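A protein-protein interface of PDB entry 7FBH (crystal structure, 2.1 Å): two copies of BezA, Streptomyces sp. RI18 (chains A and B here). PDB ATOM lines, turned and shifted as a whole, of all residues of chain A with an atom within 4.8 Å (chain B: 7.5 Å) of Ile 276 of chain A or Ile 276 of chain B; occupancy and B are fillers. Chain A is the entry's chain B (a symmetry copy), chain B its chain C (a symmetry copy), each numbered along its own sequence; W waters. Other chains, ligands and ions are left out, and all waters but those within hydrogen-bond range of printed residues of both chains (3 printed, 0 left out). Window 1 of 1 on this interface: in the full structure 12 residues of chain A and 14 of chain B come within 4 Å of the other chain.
O of Tyr 213 of chain B sits at hydrogen-bond distance from NE of Arg 272 of chain A (2.9 Å). O of Tyr 213 of chain A lies within hydrogen-bond range of NE of Arg 272 of chain B (2.8 Å). The guanidinium group (NE) of Arg 275 of chain A is in salt-bridge range of the side-chain carboxylate (OE1) of Glu 212 of chain B, 2.8 Å away.
Of chain B, only Ile 276 comes within 4 Å of Ile 276 of chain A. Ile 276 of chain B touches one residue of chain A. Of the printed residues of chain A, Tyr 213 of chain B touches Arg 272. Of the printed residues of chain B, Arg 275 of chain A touches Glu 212 (2.8 Å). Of the printed residues of chain B, Ala 280 of chain A touches Met 279 (3.5 Å). Of the printed residues of chain A, Glu 212 of chain B touches Arg 272 and Arg 275. Ser 277 of chain A touches none of the printed residues of chain B. The nearest residue of chain B that does not touch Ile 276 of chain A is Tyr 213 of chain B (4.1 Å). The nearest residue of chain A that does not touch Ile 276 of chain B is Tyr 213 of chain A (4.2 Å). The nearest printed residue of chain B that does not touch Arg 275 of chain A is Tyr 213 of chain B (4.8 Å).
Water W3 lies within hydrogen-bond range of the guanidinium group of Arg 272 of chain B (2.7 Å) and the backbone carbonyl oxygen of Tyr 213 of chain A (2.9 Å). Water W2 bridges NH2 of Arg 272 of chain A (2.8 Å) and O of Tyr 213 of chain B (2.9 Å). Water W1 lies within hydrogen-bond range of the backbone carbonyl oxygen (O) of Glu 212 of chain B (3.0 Å) and the backbone NH (N) of Arg 272 of chain A (3.3 Å).
Tyr 213 of chain A touches Arg 272 of chain B, and with the chains exchanged Arg 272 of chain A touches Tyr 213 of chain B. Ile 276 of chain A touches its own counterpart, Ile 276 of chain B. Met 279 of chain A touches Ala 280 of chain B, and with the chains exchanged Ala 280 of chain A touches Met 279 of chain B.
Among the printed residues, pairs that only touch across the chains: Arg 272 of chain A with Glu 212 of chain B, Arg 272 of chain A with Tyr 215 of chain B, Ile 276 of chain A with Ile 276 of chain B, Met 279 of chain A with Ala 280 of chain B and Ala 280 of chain A with Met 279 of chain B.
Hydrophobic or aromatic side chains of chain A within 4 Å of the printed part of chain B: Tyr 213, Ile 276, Met 279 and Ala 280. Printed residues of chain B that touch a printed residue of chain A: Glu 212, Tyr 213, Tyr 215, Arg 272, Ile 276, Met 279 and Ala 280. Hydrophobic or aromatic side chains of chain B within 4 Å of the printed part of chain A: Tyr 213, Tyr 215, Ile 276, Met 279 and Ala 280. Along chain B the printed residues that touch a printed residue of chain A span positions 212 to 280. Among the printed residues, 8 pairs touch across the chains. Among the printed residues, Asp or Glu carboxylates within 4 Å of a Lys or Arg side-chain nitrogen of the other chain: Arg 275 of chain A with Glu 212 of chain B.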
ATOM      1  N   TYR A 213     -23.033 -10.517 -17.090  1.00  0.00           N
ATOM      2  CA  TYR A 213     -22.028 -11.001 -16.157  1.00  0.00           C
ATOM      3  C   TYR A 213     -20.759 -10.145 -16.177  1.00  0.00           C
ATOM      4  O   TYR A 213     -20.097 -10.012 -15.142  1.00  0.00           O
ATOM      5  CB  TYR A 213     -21.708 -12.466 -16.472  1.00  0.00           C
ATOM      6  CG  TYR A 213     -20.766 -13.134 -15.489  1.00  0.00           C
ATOM      7  CD1 TYR A 213     -21.185 -13.459 -14.204  1.00  0.00           C
ATOM      8  CD2 TYR A 213     -19.458 -13.447 -15.851  1.00  0.00           C
ATOM      9  CE1 TYR A 213     -20.331 -14.068 -13.304  1.00  0.00           C
ATOM     10  CE2 TYR A 213     -18.601 -14.063 -14.958  1.00  0.00           C
ATOM     11  CZ  TYR A 213     -19.044 -14.366 -13.682  1.00  0.00           C
ATOM     12  OH  TYR A 213     -18.185 -14.982 -12.789  1.00  0.00           O
ATOM     13  N   ARG A 272     -17.417 -19.893  -2.863  1.00  0.00           N
ATOM     14  CA  ARG A 272     -18.694 -19.554  -3.483  1.00  0.00           C
ATOM     15  C   ARG A 272     -18.488 -18.764  -4.773  1.00  0.00           C
ATOM     16  O   ARG A 272     -19.174 -19.008  -5.774  1.00  0.00           O
ATOM     17  CB  ARG A 272     -19.552 -18.769  -2.499  1.00  0.00           C
ATOM     18  CG  ARG A 272     -20.839 -18.273  -3.109  1.00  0.00           C
ATOM     19  CD  ARG A 272     -21.767 -17.778  -2.045  1.00  0.00           C
ATOM     20  NE  ARG A 272     -23.047 -17.401  -2.615  1.00  0.00           N
ATOM     21  CZ  ARG A 272     -23.326 -16.188  -3.068  1.00  0.00           C
ATOM     22  NH1 ARG A 272     -22.409 -15.234  -3.091  1.00  0.00           N
ATOM     23  NH2 ARG A 272     -24.553 -15.926  -3.504  1.00  0.00           N
ATOM     24  N   GLN A 273     -17.529 -17.834  -4.773  1.00  0.00           N
ATOM     25  CA  GLN A 273     -17.237 -17.057  -5.975  1.00  0.00           C
ATOM     26  C   GLN A 273     -16.732 -17.945  -7.097  1.00  0.00           C
ATOM     27  O   GLN A 273     -17.116 -17.767  -8.258  1.00  0.00           O
ATOM     28  CB  GLN A 273     -16.215 -15.962  -5.667  1.00  0.00           C
ATOM     29  CG  GLN A 273     -16.828 -14.698  -5.091  1.00  0.00           C
ATOM     30  CD  GLN A 273     -15.771 -13.691  -4.656  1.00  0.00           C
ATOM     31  OE1 GLN A 273     -15.987 -12.904  -3.720  1.00  0.00           O
ATOM     32  NE2 GLN A 273     -14.623 -13.702  -5.337  1.00  0.00           N
ATOM     33  N   LEU A 274     -15.888 -18.931  -6.772  1.00  0.00           N
ATOM     34  CA  LEU A 274     -15.408 -19.844  -7.803  1.00  0.00           C
ATOM     35  C   LEU A 274     -16.535 -20.731  -8.323  1.00  0.00           C
ATOM     36  O   LEU A 274     -16.620 -20.990  -9.531  1.00  0.00           O
ATOM     37  CB  LEU A 274     -14.251 -20.680  -7.260  1.00  0.00           C
ATOM     38  CG  LEU A 274     -12.972 -19.855  -7.142  1.00  0.00           C
ATOM     39  CD1 LEU A 274     -11.938 -20.541  -6.265  1.00  0.00           C
ATOM     40  CD2 LEU A 274     -12.409 -19.588  -8.535  1.00  0.00           C
ATOM     41  N   ARG A 275     -17.415 -21.194  -7.433  1.00  0.00           N
ATOM     42  CA  ARG A 275     -18.584 -21.940  -7.889  1.00  0.00           C
ATOM     43  C   ARG A 275     -19.436 -21.098  -8.827  1.00  0.00           C
ATOM     44  O   ARG A 275     -19.901 -21.588  -9.865  1.00  0.00           O
ATOM     45  CB  ARG A 275     -19.411 -22.409  -6.685  1.00  0.00           C
ATOM     46  CG  ARG A 275     -20.811 -22.923  -7.038  1.00  0.00           C
ATOM     47  CD  ARG A 275     -20.777 -24.192  -7.868  1.00  0.00           C
ATOM     48  NE  ARG A 275     -19.951 -25.228  -7.255  1.00  0.00           N
ATOM     49  CZ  ARG A 275     -19.641 -26.381  -7.842  1.00  0.00           C
ATOM     50  NH1 ARG A 275     -20.090 -26.685  -9.052  1.00  0.00           N
ATOM     51  NH2 ARG A 275     -18.859 -27.247  -7.200  1.00  0.00           N
ATOM     52  N   ILE A 276     -19.636 -19.819  -8.486  1.00  0.00           N
ATOM     53  CA  ILE A 276     -20.358 -18.906  -9.370  1.00  0.00           C
ATOM     54  C   ILE A 276     -19.616 -18.745 -10.703  1.00  0.00           C
ATOM     55  O   ILE A 276     -20.222 -18.803 -11.783  1.00  0.00           O
ATOM     56  CB  ILE A 276     -20.594 -17.561  -8.650  1.00  0.00           C
ATOM     57  CG1 ILE A 276     -21.667 -17.733  -7.565  1.00  0.00           C
ATOM     58  CG2 ILE A 276     -20.998 -16.476  -9.641  1.00  0.00           C
ATOM     59  CD1 ILE A 276     -21.810 -16.587  -6.621  1.00  0.00           C
ATOM     60  N   SER A 277     -18.289 -18.597 -10.656  1.00  0.00           N
ATOM     61  CA  SER A 277     -17.533 -18.504 -11.904  1.00  0.00           C
ATOM     62  C   SER A 277     -17.683 -19.777 -12.739  1.00  0.00           C
ATOM     63  O   SER A 277     -17.807 -19.720 -13.973  1.00  0.00           O
ATOM     64  CB  SER A 277     -16.070 -18.208 -11.593  1.00  0.00           C
ATOM     65  OG  SER A 277     -15.313 -18.074 -12.787  1.00  0.00           O
ATOM     66  N   LEU A 278     -17.712 -20.942 -12.085  1.00  0.00           N
ATOM     67  CA  LEU A 278     -17.912 -22.179 -12.833  1.00  0.00           C
ATOM     68  C   LEU A 278     -19.269 -22.165 -13.534  1.00  0.00           C
ATOM     69  O   LEU A 278     -19.370 -22.489 -14.724  1.00  0.00           O
ATOM     70  CB  LEU A 278     -17.772 -23.390 -11.896  1.00  0.00           C
ATOM     71  CG  LEU A 278     -17.553 -24.799 -12.471  1.00  0.00           C
ATOM     72  CD1 LEU A 278     -17.281 -25.802 -11.331  1.00  0.00           C
ATOM     73  CD2 LEU A 278     -18.724 -25.297 -13.271  1.00  0.00           C
ATOM     74  N   MET A 279     -20.326 -21.777 -12.811  1.00  0.00           N
ATOM     75  CA  MET A 279     -21.659 -21.719 -13.411  1.00  0.00           C
ATOM     76  C   MET A 279     -21.707 -20.757 -14.594  1.00  0.00           C
ATOM     77  O   MET A 279     -22.282 -21.082 -15.641  1.00  0.00           O
ATOM     78  CB  MET A 279     -22.684 -21.305 -12.366  1.00  0.00           C
ATOM     79  CG  MET A 279     -22.878 -22.358 -11.306  1.00  0.00           C
ATOM     80  SD  MET A 279     -24.075 -21.898 -10.064  1.00  0.00           S
ATOM     81  CE  MET A 279     -23.346 -20.503  -9.304  1.00  0.00           C
ATOM     82  N   ALA A 280     -21.103 -19.573 -14.444  1.00  0.00           N
ATOM     83  CA  ALA A 280     -21.095 -18.590 -15.528  1.00  0.00           C
ATOM     84  C   ALA A 280     -20.311 -19.103 -16.719  1.00  0.00           C
ATOM     85  O   ALA A 280     -20.719 -18.922 -17.870  1.00  0.00           O
ATOM     86  CB  ALA A 280     -20.504 -17.265 -15.034  1.00  0.00           C
ATOM     87  N   GLU B 212     -22.006 -24.951  -1.629  1.00  0.00           N
ATOM     88  CA  GLU B 212     -21.095 -23.837  -1.869  1.00  0.00           C
ATOM     89  C   GLU B 212     -21.845 -22.545  -2.191  1.00  0.00           C
ATOM     90  O   GLU B 212     -21.398 -21.461  -1.801  1.00  0.00           O
ATOM     91  CB  GLU B 212     -20.099 -24.210  -2.975  1.00  0.00           C
ATOM     92  CG  GLU B 212     -19.117 -25.307  -2.529  1.00  0.00           C
ATOM     93  CD  GLU B 212     -18.291 -25.909  -3.672  1.00  0.00           C
ATOM     94  OE1 GLU B 212     -18.608 -25.688  -4.875  1.00  0.00           O
ATOM     95  OE2 GLU B 212     -17.301 -26.598  -3.361  1.00  0.00           O
ATOM     96  N   TYR B 213     -23.020 -22.638  -2.816  1.00  0.00           N
ATOM     97  CA  TYR B 213     -23.788 -21.426  -3.100  1.00  0.00           C
ATOM     98  C   TYR B 213     -24.500 -20.876  -1.859  1.00  0.00           C
ATOM     99  O   TYR B 213     -24.645 -19.654  -1.727  1.00  0.00           O
ATOM    100  CB  TYR B 213     -24.800 -21.690  -4.219  1.00  0.00           C
ATOM    101  CG  TYR B 213     -25.523 -20.435  -4.710  1.00  0.00           C
ATOM    102  CD1 TYR B 213     -24.833 -19.447  -5.393  1.00  0.00           C
ATOM    103  CD2 TYR B 213     -26.900 -20.273  -4.532  1.00  0.00           C
ATOM    104  CE1 TYR B 213     -25.488 -18.294  -5.862  1.00  0.00           C
ATOM    105  CE2 TYR B 213     -27.560 -19.136  -4.994  1.00  0.00           C
ATOM    106  CZ  TYR B 213     -26.849 -18.149  -5.658  1.00  0.00           C
ATOM    107  OH  TYR B 213     -27.502 -17.022  -6.129  1.00  0.00           O
ATOM    108  N   TYR B 215     -23.543 -21.649   1.460  1.00  0.00           N
ATOM    109  CA  TYR B 215     -22.674 -21.715   2.651  1.00  0.00           C
ATOM    110  C   TYR B 215     -23.160 -22.749   3.678  1.00  0.00           C
ATOM    111  O   TYR B 215     -23.007 -22.555   4.884  1.00  0.00           O
ATOM    112  CB  TYR B 215     -22.528 -20.354   3.355  1.00  0.00           C
ATOM    113  CG  TYR B 215     -21.916 -19.220   2.550  1.00  0.00           C
ATOM    114  CD1 TYR B 215     -20.636 -19.328   2.007  1.00  0.00           C
ATOM    115  CD2 TYR B 215     -22.608 -18.030   2.371  1.00  0.00           C
ATOM    116  CE1 TYR B 215     -20.073 -18.285   1.284  1.00  0.00           C
ATOM    117  CE2 TYR B 215     -22.048 -16.962   1.656  1.00  0.00           C
ATOM    118  CZ  TYR B 215     -20.779 -17.107   1.119  1.00  0.00           C
ATOM    119  OH  TYR B 215     -20.224 -16.086   0.394  1.00  0.00           O
ATOM    120  N   THR B 256     -36.943 -15.647 -12.092  1.00  0.00           N
ATOM    121  CA  THR B 256     -35.738 -14.871 -12.369  1.00  0.00           C
ATOM    122  C   THR B 256     -35.685 -14.453 -13.831  1.00  0.00           C
ATOM    123  O   THR B 256     -35.400 -13.288 -14.141  1.00  0.00           O
ATOM    124  CB  THR B 256     -34.500 -15.686 -11.980  1.00  0.00           C
ATOM    125  OG1 THR B 256     -34.679 -16.201 -10.654  1.00  0.00           O
ATOM    126  CG2 THR B 256     -33.256 -14.810 -11.985  1.00  0.00           C
ATOM    127  N   LEU B 260     -35.654 -10.563 -15.353  1.00  0.00           N
ATOM    128  CA  LEU B 260     -34.613 -10.089 -16.266  1.00  0.00           C
ATOM    129  C   LEU B 260     -35.208  -9.612 -17.586  1.00  0.00           C
ATOM    130  O   LEU B 260     -34.737  -8.624 -18.167  1.00  0.00           O
ATOM    131  CB  LEU B 260     -33.587 -11.195 -16.515  1.00  0.00           C
ATOM    132  CG  LEU B 260     -32.684 -11.588 -15.346  1.00  0.00           C
ATOM    133  CD1 LEU B 260     -32.261 -13.063 -15.489  1.00  0.00           C
ATOM    134  CD2 LEU B 260     -31.462 -10.687 -15.281  1.00  0.00           C
ATOM    135  N   VAL B 269     -25.597  -3.738 -11.444  1.00  0.00           N
ATOM    136  CA  VAL B 269     -25.217  -4.643 -10.365  1.00  0.00           C
ATOM    137  C   VAL B 269     -26.363  -5.589 -10.020  1.00  0.00           C
ATOM    138  O   VAL B 269     -26.153  -6.795  -9.846  1.00  0.00           O
ATOM    139  CB  VAL B 269     -24.752  -3.836  -9.136  1.00  0.00           C
ATOM    140  CG1 VAL B 269     -24.620  -4.744  -7.924  1.00  0.00           C
ATOM    141  CG2 VAL B 269     -23.415  -3.158  -9.420  1.00  0.00           C
ATOM    142  N   ASP B 270     -27.590  -5.066  -9.910  1.00  0.00           N
ATOM    143  CA  ASP B 270     -28.721  -5.938  -9.579  1.00  0.00           C
ATOM    144  C   ASP B 270     -29.046  -6.885 -10.723  1.00  0.00           C
ATOM    145  O   ASP B 270     -29.449  -8.034 -10.482  1.00  0.00           O
ATOM    146  CB  ASP B 270     -29.954  -5.114  -9.217  1.00  0.00           C
ATOM    147  CG  ASP B 270     -29.791  -4.378  -7.902  1.00  0.00           C
ATOM    148  OD1 ASP B 270     -28.893  -4.764  -7.118  1.00  0.00           O
ATOM    149  OD2 ASP B 270     -30.558  -3.423  -7.646  1.00  0.00           O
ATOM    150  N   ARG B 271     -28.870  -6.419 -11.967  1.00  0.00           N
ATOM    151  CA  ARG B 271     -29.074  -7.290 -13.115  1.00  0.00           C
ATOM    152  C   ARG B 271     -28.061  -8.429 -13.126  1.00  0.00           C
ATOM    153  O   ARG B 271     -28.429  -9.582 -13.374  1.00  0.00           O
ATOM    154  CB  ARG B 271     -29.003  -6.495 -14.419  1.00  0.00           C
ATOM    155  CG  ARG B 271     -29.104  -7.375 -15.668  1.00  0.00           C
ATOM    156  CD  ARG B 271     -29.460  -6.559 -16.927  1.00  0.00           C
ATOM    157  NE  ARG B 271     -30.783  -5.944 -16.854  1.00  0.00           N
ATOM    158  CZ  ARG B 271     -31.916  -6.525 -17.236  1.00  0.00           C
ATOM    159  NH1 ARG B 271     -31.938  -7.756 -17.731  1.00  0.00           N
ATOM    160  NH2 ARG B 271     -33.062  -5.855 -17.116  1.00  0.00           N
ATOM    161  N   ARG B 272     -26.785  -8.130 -12.840  1.00  0.00           N
ATOM    162  CA  ARG B 272     -25.784  -9.195 -12.736  1.00  0.00           C
ATOM    163  C   ARG B 272     -26.106 -10.164 -11.601  1.00  0.00           C
ATOM    164  O   ARG B 272     -25.906 -11.379 -11.735  1.00  0.00           O
ATOM    165  CB  ARG B 272     -24.389  -8.606 -12.534  1.00  0.00           C
ATOM    166  CG  ARG B 272     -23.309  -9.663 -12.345  1.00  0.00           C
ATOM    167  CD  ARG B 272     -21.905  -9.051 -12.532  1.00  0.00           C
ATOM    168  NE  ARG B 272     -20.846 -10.055 -12.448  1.00  0.00           N
ATOM    169  CZ  ARG B 272     -20.350 -10.510 -11.306  1.00  0.00           C
ATOM    170  NH1 ARG B 272     -20.838 -10.125 -10.141  1.00  0.00           N
ATOM    171  NH2 ARG B 272     -19.333 -11.364 -11.333  1.00  0.00           N
ATOM    172  N   GLN B 273     -26.576  -9.641 -10.464  1.00  0.00           N
ATOM    173  CA  GLN B 273     -26.945 -10.508  -9.351  1.00  0.00           C
ATOM    174  C   GLN B 273     -28.073 -11.445  -9.743  1.00  0.00           C
ATOM    175  O   GLN B 273     -28.074 -12.619  -9.352  1.00  0.00           O
ATOM    176  CB  GLN B 273     -27.363  -9.673  -8.143  1.00  0.00           C
ATOM    177  CG  GLN B 273     -26.265  -9.444  -7.140  1.00  0.00           C
ATOM    178  CD  GLN B 273     -26.735  -8.603  -5.960  1.00  0.00           C
ATOM    179  OE1 GLN B 273     -27.847  -8.789  -5.438  1.00  0.00           O
ATOM    180  NE2 GLN B 273     -25.891  -7.661  -5.537  1.00  0.00           N
ATOM    181  N   LEU B 274     -29.045 -10.948 -10.512  1.00  0.00           N
ATOM    182  CA  LEU B 274     -30.149 -11.809 -10.916  1.00  0.00           C
ATOM    183  C   LEU B 274     -29.709 -12.812 -11.967  1.00  0.00           C
ATOM    184  O   LEU B 274     -30.187 -13.953 -11.968  1.00  0.00           O
ATOM    185  CB  LEU B 274     -31.319 -10.984 -11.436  1.00  0.00           C
ATOM    186  CG  LEU B 274     -32.192 -10.436 -10.311  1.00  0.00           C
ATOM    187  CD1 LEU B 274     -32.940  -9.239 -10.823  1.00  0.00           C
ATOM    188  CD2 LEU B 274     -33.144 -11.496  -9.805  1.00  0.00           C
ATOM    189  N   ARG B 275     -28.788 -12.417 -12.852  1.00  0.00           N
ATOM    190  CA  ARG B 275     -28.270 -13.364 -13.830  1.00  0.00           C
ATOM    191  C   ARG B 275     -27.505 -14.487 -13.139  1.00  0.00           C
ATOM    192  O   ARG B 275     -27.597 -15.651 -13.541  1.00  0.00           O
ATOM    193  CB  ARG B 275     -27.400 -12.618 -14.850  1.00  0.00           C
ATOM    194  CG  ARG B 275     -26.537 -13.490 -15.721  1.00  0.00           C
ATOM    195  CD  ARG B 275     -27.350 -14.409 -16.638  1.00  0.00           C
ATOM    196  NE  ARG B 275     -28.273 -13.656 -17.478  1.00  0.00           N
ATOM    197  CZ  ARG B 275     -29.114 -14.204 -18.345  1.00  0.00           C
ATOM    198  NH1 ARG B 275     -29.171 -15.516 -18.518  1.00  0.00           N
ATOM    199  NH2 ARG B 275     -29.912 -13.412 -19.070  1.00  0.00           N
ATOM    200  N   ILE B 276     -26.776 -14.167 -12.071  1.00  0.00           N
ATOM    201  CA  ILE B 276     -26.096 -15.214 -11.303  1.00  0.00           C
ATOM    202  C   ILE B 276     -27.110 -16.113 -10.603  1.00  0.00           C
ATOM    203  O   ILE B 276     -26.933 -17.340 -10.531  1.00  0.00           O
ATOM    204  CB  ILE B 276     -25.105 -14.579 -10.308  1.00  0.00           C
ATOM    205  CG1 ILE B 276     -23.880 -14.065 -11.088  1.00  0.00           C
ATOM    206  CG2 ILE B 276     -24.688 -15.603  -9.202  1.00  0.00           C
ATOM    207  CD1 ILE B 276     -23.092 -13.000 -10.363  1.00  0.00           C
ATOM    208  N   SER B 277     -28.194 -15.526 -10.090  1.00  0.00           N
ATOM    209  CA  SER B 277     -29.211 -16.338  -9.430  1.00  0.00           C
ATOM    210  C   SER B 277     -29.843 -17.309 -10.417  1.00  0.00           C
ATOM    211  O   SER B 277     -30.124 -18.468 -10.075  1.00  0.00           O
ATOM    212  CB  SER B 277     -30.269 -15.432  -8.795  1.00  0.00           C
ATOM    213  OG  SER B 277     -31.182 -16.177  -8.015  1.00  0.00           O
ATOM    214  N   LEU B 278     -30.083 -16.839 -11.650  1.00  0.00           N
ATOM    215  CA  LEU B 278     -30.639 -17.691 -12.697  1.00  0.00           C
ATOM    216  C   LEU B 278     -29.726 -18.879 -12.983  1.00  0.00           C
ATOM    217  O   LEU B 278     -30.178 -20.029 -13.013  1.00  0.00           O
ATOM    218  CB  LEU B 278     -30.869 -16.868 -13.967  1.00  0.00           C
ATOM    219  CG  LEU B 278     -31.296 -17.626 -15.225  1.00  0.00           C
ATOM    220  CD1 LEU B 278     -32.476 -18.487 -14.919  1.00  0.00           C
ATOM    221  CD2 LEU B 278     -31.656 -16.661 -16.349  1.00  0.00           C
ATOM    222  N   MET B 279     -28.439 -18.617 -13.217  1.00  0.00           N
ATOM    223  CA  MET B 279     -27.482 -19.701 -13.419  1.00  0.00           C
ATOM    224  C   MET B 279     -27.461 -20.641 -12.225  1.00  0.00           C
ATOM    225  O   MET B 279     -27.389 -21.862 -12.390  1.00  0.00           O
ATOM    226  CB  MET B 279     -26.077 -19.144 -13.642  1.00  0.00           C
ATOM    227  CG  MET B 279     -25.948 -18.134 -14.763  1.00  0.00           C
ATOM    228  SD  MET B 279     -24.276 -17.446 -14.797  1.00  0.00           S
ATOM    229  CE  MET B 279     -24.494 -15.733 -14.474  1.00  0.00           C
ATOM    230  N   ALA B 280     -27.483 -20.086 -11.005  1.00  0.00           N
ATOM    231  CA  ALA B 280     -27.410 -20.936  -9.825  1.00  0.00           C
ATOM    232  C   ALA B 280     -28.659 -21.788  -9.721  1.00  0.00           C
ATOM    233  O   ALA B 280     -28.579 -22.984  -9.418  1.00  0.00           O
ATOM    234  CB  ALA B 280     -27.221 -20.097  -8.560  1.00  0.00           C
ATOM    235  N   ASN B 281     -29.816 -21.192 -10.024  1.00  0.00           N
ATOM    236  CA  ASN B 281     -31.069 -21.934  -9.987  1.00  0.00           C
ATOM    237  C   ASN B 281     -31.064 -23.099 -10.968  1.00  0.00           C
ATOM    238  O   ASN B 281     -31.588 -24.173 -10.664  1.00  0.00           O
ATOM    239  CB  ASN B 281     -32.234 -20.984 -10.270  1.00  0.00           C
ATOM    240  CG  ASN B 281     -32.803 -20.432  -9.027  1.00  0.00           C
ATOM    241  OD1 ASN B 281     -33.702 -21.028  -8.451  1.00  0.00           O
ATOM    242  ND2 ASN B 281     -32.259 -19.306  -8.557  1.00  0.00           N
ATOM    243  N   GLN B 282     -30.481 -22.915 -12.146  1.00  0.00           N
ATOM    244  CA  GLN B 282     -30.391 -24.036 -13.078  1.00  0.00           C
ATOM    245  C   GLN B 282     -29.407 -25.096 -12.577  1.00  0.00           C
ATOM    246  O   GLN B 282     -29.705 -26.295 -12.629  1.00  0.00           O
ATOM    247  CB  GLN B 282     -30.000 -23.529 -14.461  1.00  0.00           C
ATOM    248  CG  GLN B 282     -31.070 -22.613 -15.057  1.00  0.00           C
ATOM    249  CD  GLN B 282     -30.611 -21.917 -16.311  1.00  0.00           C
ATOM    250  OE1 GLN B 282     -29.434 -21.596 -16.458  1.00  0.00           O
ATOM    251  NE2 GLN B 282     -31.538 -21.670 -17.225  1.00  0.00           N
HETATM  252  O   HOH W   1     -18.778 -21.748  -0.438  1.00  0.00           O
HETATM  253  O   HOH W   2     -26.506 -17.444  -2.226  1.00  0.00           O
HETATM  254  O   HOH W   3     -17.911 -10.905 -13.525  1.00  0.00           O
